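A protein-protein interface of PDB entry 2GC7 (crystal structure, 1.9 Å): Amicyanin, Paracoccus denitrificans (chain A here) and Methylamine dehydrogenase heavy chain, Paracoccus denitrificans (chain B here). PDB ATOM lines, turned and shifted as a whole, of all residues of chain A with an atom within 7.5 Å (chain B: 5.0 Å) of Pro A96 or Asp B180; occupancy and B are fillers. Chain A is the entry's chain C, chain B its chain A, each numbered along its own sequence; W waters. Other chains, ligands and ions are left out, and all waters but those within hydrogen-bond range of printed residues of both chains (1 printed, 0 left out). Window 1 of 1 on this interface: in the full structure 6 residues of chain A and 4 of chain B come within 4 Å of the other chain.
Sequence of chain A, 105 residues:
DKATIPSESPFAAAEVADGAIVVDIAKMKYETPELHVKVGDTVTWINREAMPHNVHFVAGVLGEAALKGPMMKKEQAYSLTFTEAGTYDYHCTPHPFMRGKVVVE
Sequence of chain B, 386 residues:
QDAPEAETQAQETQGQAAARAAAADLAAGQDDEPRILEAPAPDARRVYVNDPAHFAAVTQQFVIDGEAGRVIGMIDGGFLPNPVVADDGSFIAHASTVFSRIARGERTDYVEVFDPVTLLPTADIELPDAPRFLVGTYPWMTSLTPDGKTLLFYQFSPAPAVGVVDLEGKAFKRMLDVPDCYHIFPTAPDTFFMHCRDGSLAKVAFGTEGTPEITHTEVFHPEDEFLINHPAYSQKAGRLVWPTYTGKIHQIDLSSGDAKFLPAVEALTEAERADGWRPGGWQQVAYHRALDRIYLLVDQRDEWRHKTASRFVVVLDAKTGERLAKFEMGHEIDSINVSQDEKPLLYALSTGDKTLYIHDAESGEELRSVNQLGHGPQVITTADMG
Pro A96 touches just these residues of chain B: Phe B156 and Asp B180. Printed residues of chain B within 4 Å of Pro A94: Phe B156 (3.8 Å). Printed residues of chain B within 4 Å of His A91: Pro B158. Of the printed residues of chain A, Pro B158 touches His A91 (3.0 Å). Cys A92 touches none of the printed residues of chain B. The nearest residue of chain B that does not touch Pro A96 is Pro B160 (4.4 Å). The nearest residue of chain A that does not touch Asp B180 is Met A98 (5.7 Å).
The backbone NH (N) of Arg B197 lies within hydrogen-bond range of the backbone carbonyl oxygen (O) of Asp B180 (3.1 Å). O of Pro A96 is in hydrogen-bond range of NH2 of Arg A99, at 2.7 Å. The side-chain sulfur (SG) of Cys B181 is disulfide-bonded to the side-chain sulfur (SG) of Cys B196 (2.0 Å).
NE2 of His A91 is in hydrogen-bond range of O of Pro B158. OD2 of Asp B180 lies within salt-bridge range of NH1 of Arg A99 (2.6 Å).
Among the printed residues, merely in contact across the chains: Pro A94 with Phe B156 (3.8 Å), Pro A96 with Phe B156 (3.6 Å), Pro A96 with Asp B180 (3.9 Å), Phe A97 with Asp B180 (3.5 Å) and Phe A97 with Arg B197 (3.4 Å).
Water W1 lies within hydrogen-bond range of O of Thr A93, NE2 of His A91 and O of Pro B158.
Of the 11 printed residues of chain B, 4 touch a printed residue of chain A. Printed residues of chain B that touch a printed residue of chain A: Phe B156, Pro B158, Asp B180 and Arg B197. Hydrophobic or aromatic side chains of chain B that line the printed part of chain A: Phe B156. Of the 10 printed residues of chain A, 5 touch a printed residue of chain B. Hydrophobic or aromatic side chains of chain A that line the printed part of chain B: His A91, Pro A96 and Phe A97. Among the printed residues, Asp or Glu carboxylates within 4 Å of a Lys or Arg side-chain nitrogen of the other chain: Arg A99 with Asp B180 (2.6 Å).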
ATOM      1  N   TYR A  90      14.293   5.680   6.094  1.00  0.00           N
ATOM      2  CA  TYR A  90      14.882   6.983   5.821  1.00  0.00           C
ATOM      3  C   TYR A  90      13.850   8.072   6.084  1.00  0.00           C
ATOM      4  O   TYR A  90      12.668   7.779   6.284  1.00  0.00           O
ATOM      5  CB  TYR A  90      15.372   7.070   4.368  1.00  0.00           C
ATOM      6  CG  TYR A  90      14.284   6.928   3.321  1.00  0.00           C
ATOM      7  CD1 TYR A  90      13.809   5.670   2.938  1.00  0.00           C
ATOM      8  CD2 TYR A  90      13.734   8.054   2.705  1.00  0.00           C
ATOM      9  CE1 TYR A  90      12.812   5.539   1.963  1.00  0.00           C
ATOM     10  CE2 TYR A  90      12.738   7.936   1.731  1.00  0.00           C
ATOM     11  CZ  TYR A  90      12.284   6.678   1.364  1.00  0.00           C
ATOM     12  OH  TYR A  90      11.309   6.565   0.399  1.00  0.00           O
ATOM     13  N   HIS A  91      14.312   9.319   6.099  1.00  0.00           N
ATOM     14  CA  HIS A  91      13.447  10.472   6.321  1.00  0.00           C
ATOM     15  C   HIS A  91      14.067  11.674   5.624  1.00  0.00           C
ATOM     16  O   HIS A  91      15.152  11.578   5.057  1.00  0.00           O
ATOM     17  CB  HIS A  91      13.303  10.775   7.822  1.00  0.00           C
ATOM     18  CG  HIS A  91      14.557  11.297   8.461  1.00  0.00           C
ATOM     19  ND1 HIS A  91      15.623  10.485   8.783  1.00  0.00           N
ATOM     20  CD2 HIS A  91      14.925  12.553   8.808  1.00  0.00           C
ATOM     21  CE1 HIS A  91      16.594  11.217   9.300  1.00  0.00           C
ATOM     22  NE2 HIS A  91      16.197  12.476   9.325  1.00  0.00           N
ATOM     23  N   CYS A  92      13.368  12.803   5.665  1.00  0.00           N
ATOM     24  CA  CYS A  92      13.856  14.035   5.061  1.00  0.00           C
ATOM     25  C   CYS A  92      14.493  14.851   6.188  1.00  0.00           C
ATOM     26  O   CYS A  92      13.847  15.136   7.194  1.00  0.00           O
ATOM     27  CB  CYS A  92      12.692  14.805   4.446  1.00  0.00           C
ATOM     28  SG  CYS A  92      13.194  16.292   3.589  1.00  0.00           S
ATOM     29  N   THR A  93      15.757  15.225   6.010  1.00  0.00           N
ATOM     30  CA  THR A  93      16.496  15.962   7.034  1.00  0.00           C
ATOM     31  C   THR A  93      15.748  17.099   7.746  1.00  0.00           C
ATOM     32  O   THR A  93      15.568  17.046   8.958  1.00  0.00           O
ATOM     33  CB  THR A  93      17.830  16.482   6.459  1.00  0.00           C
ATOM     34  OG1 THR A  93      18.614  15.364   6.021  1.00  0.00           O
ATOM     35  CG2 THR A  93      18.611  17.258   7.514  1.00  0.00           C
ATOM     36  N   PRO A  94      15.299  18.134   7.013  1.00  0.00           N
ATOM     37  CA  PRO A  94      14.582  19.231   7.682  1.00  0.00           C
ATOM     38  C   PRO A  94      13.132  18.908   8.051  1.00  0.00           C
ATOM     39  O   PRO A  94      12.493  19.654   8.797  1.00  0.00           O
ATOM     40  CB  PRO A  94      14.665  20.363   6.664  1.00  0.00           C
ATOM     41  CG  PRO A  94      14.574  19.623   5.365  1.00  0.00           C
ATOM     42  CD  PRO A  94      15.500  18.437   5.584  1.00  0.00           C
ATOM     43  N   HIS A  95      12.620  17.799   7.526  1.00  0.00           N
ATOM     44  CA  HIS A  95      11.237  17.384   7.773  1.00  0.00           C
ATOM     45  C   HIS A  95      11.235  15.962   8.333  1.00  0.00           C
ATOM     46  O   HIS A  95      10.842  15.018   7.648  1.00  0.00           O
ATOM     47  CB  HIS A  95      10.457  17.423   6.458  1.00  0.00           C
ATOM     48  CG  HIS A  95      10.709  18.656   5.645  1.00  0.00           C
ATOM     49  ND1 HIS A  95      10.779  18.676   4.269  1.00  0.00           N
ATOM     50  CD2 HIS A  95      10.895  19.942   6.038  1.00  0.00           C
ATOM     51  CE1 HIS A  95      11.000  19.941   3.884  1.00  0.00           C
ATOM     52  NE2 HIS A  95      11.078  20.748   4.925  1.00  0.00           N
ATOM     53  N   PRO A  96      11.667  15.799   9.596  1.00  0.00           N
ATOM     54  CA  PRO A  96      11.739  14.504  10.287  1.00  0.00           C
ATOM     55  C   PRO A  96      10.450  13.682  10.255  1.00  0.00           C
ATOM     56  O   PRO A  96      10.486  12.456  10.374  1.00  0.00           O
ATOM     57  CB  PRO A  96      12.138  14.892  11.713  1.00  0.00           C
ATOM     58  CG  PRO A  96      12.915  16.164  11.509  1.00  0.00           C
ATOM     59  CD  PRO A  96      12.063  16.892  10.500  1.00  0.00           C
ATOM     60  N   PHE A  97       9.318  14.359  10.102  1.00  0.00           N
ATOM     61  CA  PHE A  97       8.029  13.684  10.054  1.00  0.00           C
ATOM     62  C   PHE A  97       7.797  12.942   8.741  1.00  0.00           C
ATOM     63  O   PHE A  97       6.891  12.112   8.650  1.00  0.00           O
ATOM     64  CB  PHE A  97       6.897  14.684  10.274  1.00  0.00           C
ATOM     65  CG  PHE A  97       7.007  15.913   9.426  1.00  0.00           C
ATOM     66  CD1 PHE A  97       7.881  16.937   9.776  1.00  0.00           C
ATOM     67  CD2 PHE A  97       6.257  16.039   8.262  1.00  0.00           C
ATOM     68  CE1 PHE A  97       8.007  18.069   8.974  1.00  0.00           C
ATOM     69  CE2 PHE A  97       6.376  17.166   7.454  1.00  0.00           C
ATOM     70  CZ  PHE A  97       7.254  18.182   7.811  1.00  0.00           C
ATOM     71  N   MET A  98       8.595  13.252   7.721  1.00  0.00           N
ATOM     72  CA  MET A  98       8.477  12.579   6.422  1.00  0.00           C
ATOM     73  C   MET A  98       9.308  11.308   6.482  1.00  0.00           C
ATOM     74  O   MET A  98      10.534  11.372   6.583  1.00  0.00           O
ATOM     75  CB  MET A  98       9.029  13.449   5.298  1.00  0.00           C
ATOM     76  CG  MET A  98       8.085  14.476   4.757  1.00  0.00           C
ATOM     77  SD  MET A  98       8.922  15.478   3.516  1.00  0.00           S
ATOM     78  CE  MET A  98       8.957  14.350   2.089  1.00  0.00           C
ATOM     79  N   ARG A  99       8.647  10.161   6.405  1.00  0.00           N
ATOM     80  CA  ARG A  99       9.340   8.883   6.479  1.00  0.00           C
ATOM     81  C   ARG A  99       9.046   7.971   5.293  1.00  0.00           C
ATOM     82  O   ARG A  99       7.950   7.979   4.732  1.00  0.00           O
ATOM     83  CB  ARG A  99       8.955   8.149   7.762  1.00  0.00           C
ATOM     84  CG  ARG A  99      10.099   7.938   8.739  1.00  0.00           C
ATOM     85  CD  ARG A  99      10.177   9.042   9.770  1.00  0.00           C
ATOM     86  NE  ARG A  99       8.892   9.227  10.436  1.00  0.00           N
ATOM     87  CZ  ARG A  99       8.710   9.963  11.528  1.00  0.00           C
ATOM     88  NH1 ARG A  99       7.500  10.077  12.055  1.00  0.00           N
ATOM     89  NH2 ARG A  99       9.740  10.574  12.104  1.00  0.00           N
ATOM     90  N   PHE B 156      15.980  17.318  17.906  1.00  0.00           N
ATOM     91  CA  PHE B 156      15.177  17.457  16.700  1.00  0.00           C
ATOM     92  C   PHE B 156      15.601  16.485  15.613  1.00  0.00           C
ATOM     93  O   PHE B 156      14.778  15.753  15.061  1.00  0.00           O
ATOM     94  CB  PHE B 156      15.295  18.886  16.166  1.00  0.00           C
ATOM     95  CG  PHE B 156      14.524  19.139  14.901  1.00  0.00           C
ATOM     96  CD1 PHE B 156      13.136  19.220  14.919  1.00  0.00           C
ATOM     97  CD2 PHE B 156      15.189  19.317  13.692  1.00  0.00           C
ATOM     98  CE1 PHE B 156      12.420  19.478  13.747  1.00  0.00           C
ATOM     99  CE2 PHE B 156      14.482  19.575  12.515  1.00  0.00           C
ATOM    100  CZ  PHE B 156      13.100  19.655  12.543  1.00  0.00           C
ATOM    101  N   PRO B 158      18.674  13.519  14.261  1.00  0.00           N
ATOM    102  CA  PRO B 158      17.995  13.016  13.060  1.00  0.00           C
ATOM    103  C   PRO B 158      16.565  12.531  13.285  1.00  0.00           C
ATOM    104  O   PRO B 158      15.825  12.297  12.331  1.00  0.00           O
ATOM    105  CB  PRO B 158      18.915  11.893  12.597  1.00  0.00           C
ATOM    106  CG  PRO B 158      19.424  11.344  13.897  1.00  0.00           C
ATOM    107  CD  PRO B 158      19.752  12.600  14.672  1.00  0.00           C
ATOM    108  N   PRO B 160      13.068  12.780  16.333  1.00  0.00           N
ATOM    109  CA  PRO B 160      12.537  13.341  17.577  1.00  0.00           C
ATOM    110  C   PRO B 160      12.934  12.434  18.736  1.00  0.00           C
ATOM    111  O   PRO B 160      12.762  11.216  18.657  1.00  0.00           O
ATOM    112  CB  PRO B 160      11.028  13.330  17.347  1.00  0.00           C
ATOM    113  CG  PRO B 160      10.905  13.432  15.857  1.00  0.00           C
ATOM    114  CD  PRO B 160      11.982  12.503  15.377  1.00  0.00           C
ATOM    115  N   VAL B 178      10.511   9.445  20.709  1.00  0.00           N
ATOM    116  CA  VAL B 178       9.141   9.921  20.800  1.00  0.00           C
ATOM    117  C   VAL B 178       8.600  10.222  19.410  1.00  0.00           C
ATOM    118  O   VAL B 178       9.357  10.267  18.438  1.00  0.00           O
ATOM    119  CB  VAL B 178       9.054  11.208  21.667  1.00  0.00           C
ATOM    120  CG1 VAL B 178       9.639  10.945  23.045  1.00  0.00           C
ATOM    121  CG2 VAL B 178       9.794  12.359  20.989  1.00  0.00           C
ATOM    122  N   PRO B 179       7.276  10.411  19.292  1.00  0.00           N
ATOM    123  CA  PRO B 179       6.661  10.713  17.998  1.00  0.00           C
ATOM    124  C   PRO B 179       7.052  12.130  17.575  1.00  0.00           C
ATOM    125  O   PRO B 179       7.851  12.789  18.250  1.00  0.00           O
ATOM    126  CB  PRO B 179       5.164  10.605  18.287  1.00  0.00           C
ATOM    127  CG  PRO B 179       5.093   9.690  19.484  1.00  0.00           C
ATOM    128  CD  PRO B 179       6.244  10.170  20.316  1.00  0.00           C
ATOM    129  N   ASP B 180       6.488  12.596  16.466  1.00  0.00           N
ATOM    130  CA  ASP B 180       6.770  13.934  15.970  1.00  0.00           C
ATOM    131  C   ASP B 180       6.046  14.954  16.847  1.00  0.00           C
ATOM    132  O   ASP B 180       5.006  15.500  16.461  1.00  0.00           O
ATOM    133  CB  ASP B 180       6.305  14.067  14.521  1.00  0.00           C
ATOM    134  CG  ASP B 180       7.038  13.123  13.590  1.00  0.00           C
ATOM    135  OD1 ASP B 180       8.284  13.197  13.531  1.00  0.00           O
ATOM    136  OD2 ASP B 180       6.371  12.309  12.920  1.00  0.00           O
ATOM    137  N   CYS B 181       6.605  15.198  18.027  1.00  0.00           N
ATOM    138  CA  CYS B 181       6.031  16.128  18.986  1.00  0.00           C
ATOM    139  C   CYS B 181       7.142  17.042  19.501  1.00  0.00           C
ATOM    140  O   CYS B 181       8.324  16.706  19.390  1.00  0.00           O
ATOM    141  CB  CYS B 181       5.390  15.345  20.134  1.00  0.00           C
ATOM    142  SG  CYS B 181       4.311  13.997  19.545  1.00  0.00           S
ATOM    143  N   TYR B 182       6.746  18.181  20.076  1.00  0.00           N
ATOM    144  CA  TYR B 182       7.680  19.194  20.550  1.00  0.00           C
ATOM    145  C   TYR B 182       7.354  19.740  21.938  1.00  0.00           C
ATOM    146  O   TYR B 182       6.203  19.733  22.360  1.00  0.00           O
ATOM    147  CB  TYR B 182       7.719  20.338  19.528  1.00  0.00           C
ATOM    148  CG  TYR B 182       7.828  19.829  18.107  1.00  0.00           C
ATOM    149  CD1 TYR B 182       6.737  19.227  17.477  1.00  0.00           C
ATOM    150  CD2 TYR B 182       9.046  19.851  17.433  1.00  0.00           C
ATOM    151  CE1 TYR B 182       6.859  18.648  16.214  1.00  0.00           C
ATOM    152  CE2 TYR B 182       9.179  19.279  16.167  1.00  0.00           C
ATOM    153  CZ  TYR B 182       8.084  18.677  15.567  1.00  0.00           C
ATOM    154  OH  TYR B 182       8.214  18.100  14.323  1.00  0.00           O
ATOM    155  N   HIS B 195       3.682  18.379  22.716  1.00  0.00           N
ATOM    156  CA  HIS B 195       2.650  18.825  21.785  1.00  0.00           C
ATOM    157  C   HIS B 195       3.062  18.285  20.421  1.00  0.00           C
ATOM    158  O   HIS B 195       4.193  18.498  19.977  1.00  0.00           O
ATOM    159  CB  HIS B 195       2.559  20.350  21.748  1.00  0.00           C
ATOM    160  CG  HIS B 195       1.713  20.867  20.626  1.00  0.00           C
ATOM    161  ND1 HIS B 195       2.209  21.693  19.640  1.00  0.00           N
ATOM    162  CD2 HIS B 195       0.416  20.638  20.309  1.00  0.00           C
ATOM    163  CE1 HIS B 195       1.254  21.948  18.762  1.00  0.00           C
ATOM    164  NE2 HIS B 195       0.157  21.320  19.145  1.00  0.00           N
ATOM    165  N   CYS B 196       2.144  17.593  19.753  1.00  0.00           N
ATOM    166  CA  CYS B 196       2.454  16.979  18.468  1.00  0.00           C
ATOM    167  C   CYS B 196       1.954  17.716  17.228  1.00  0.00           C
ATOM    168  O   CYS B 196       1.024  18.522  17.291  1.00  0.00           O
ATOM    169  CB  CYS B 196       1.932  15.542  18.470  1.00  0.00           C
ATOM    170  SG  CYS B 196       2.426  14.618  19.959  1.00  0.00           S
ATOM    171  N   ARG B 197       2.588  17.422  16.098  1.00  0.00           N
ATOM    172  CA  ARG B 197       2.239  18.032  14.820  1.00  0.00           C
ATOM    173  C   ARG B 197       0.772  17.817  14.438  1.00  0.00           C
ATOM    174  O   ARG B 197       0.174  18.669  13.785  1.00  0.00           O
ATOM    175  CB  ARG B 197       3.149  17.476  13.714  1.00  0.00           C
ATOM    176  CG  ARG B 197       2.969  18.133  12.339  1.00  0.00           C
ATOM    177  CD  ARG B 197       3.775  17.394  11.270  1.00  0.00           C
ATOM    178  NE  ARG B 197       3.542  17.914   9.920  1.00  0.00           N
ATOM    179  CZ  ARG B 197       4.181  18.954   9.389  1.00  0.00           C
ATOM    180  NH1 ARG B 197       3.894  19.352   8.155  1.00  0.00           N
ATOM    181  NH2 ARG B 197       5.117  19.591  10.083  1.00  0.00           N
HETATM  182  O   HOH W   1      16.795  15.054  10.473  1.00  0.00           O
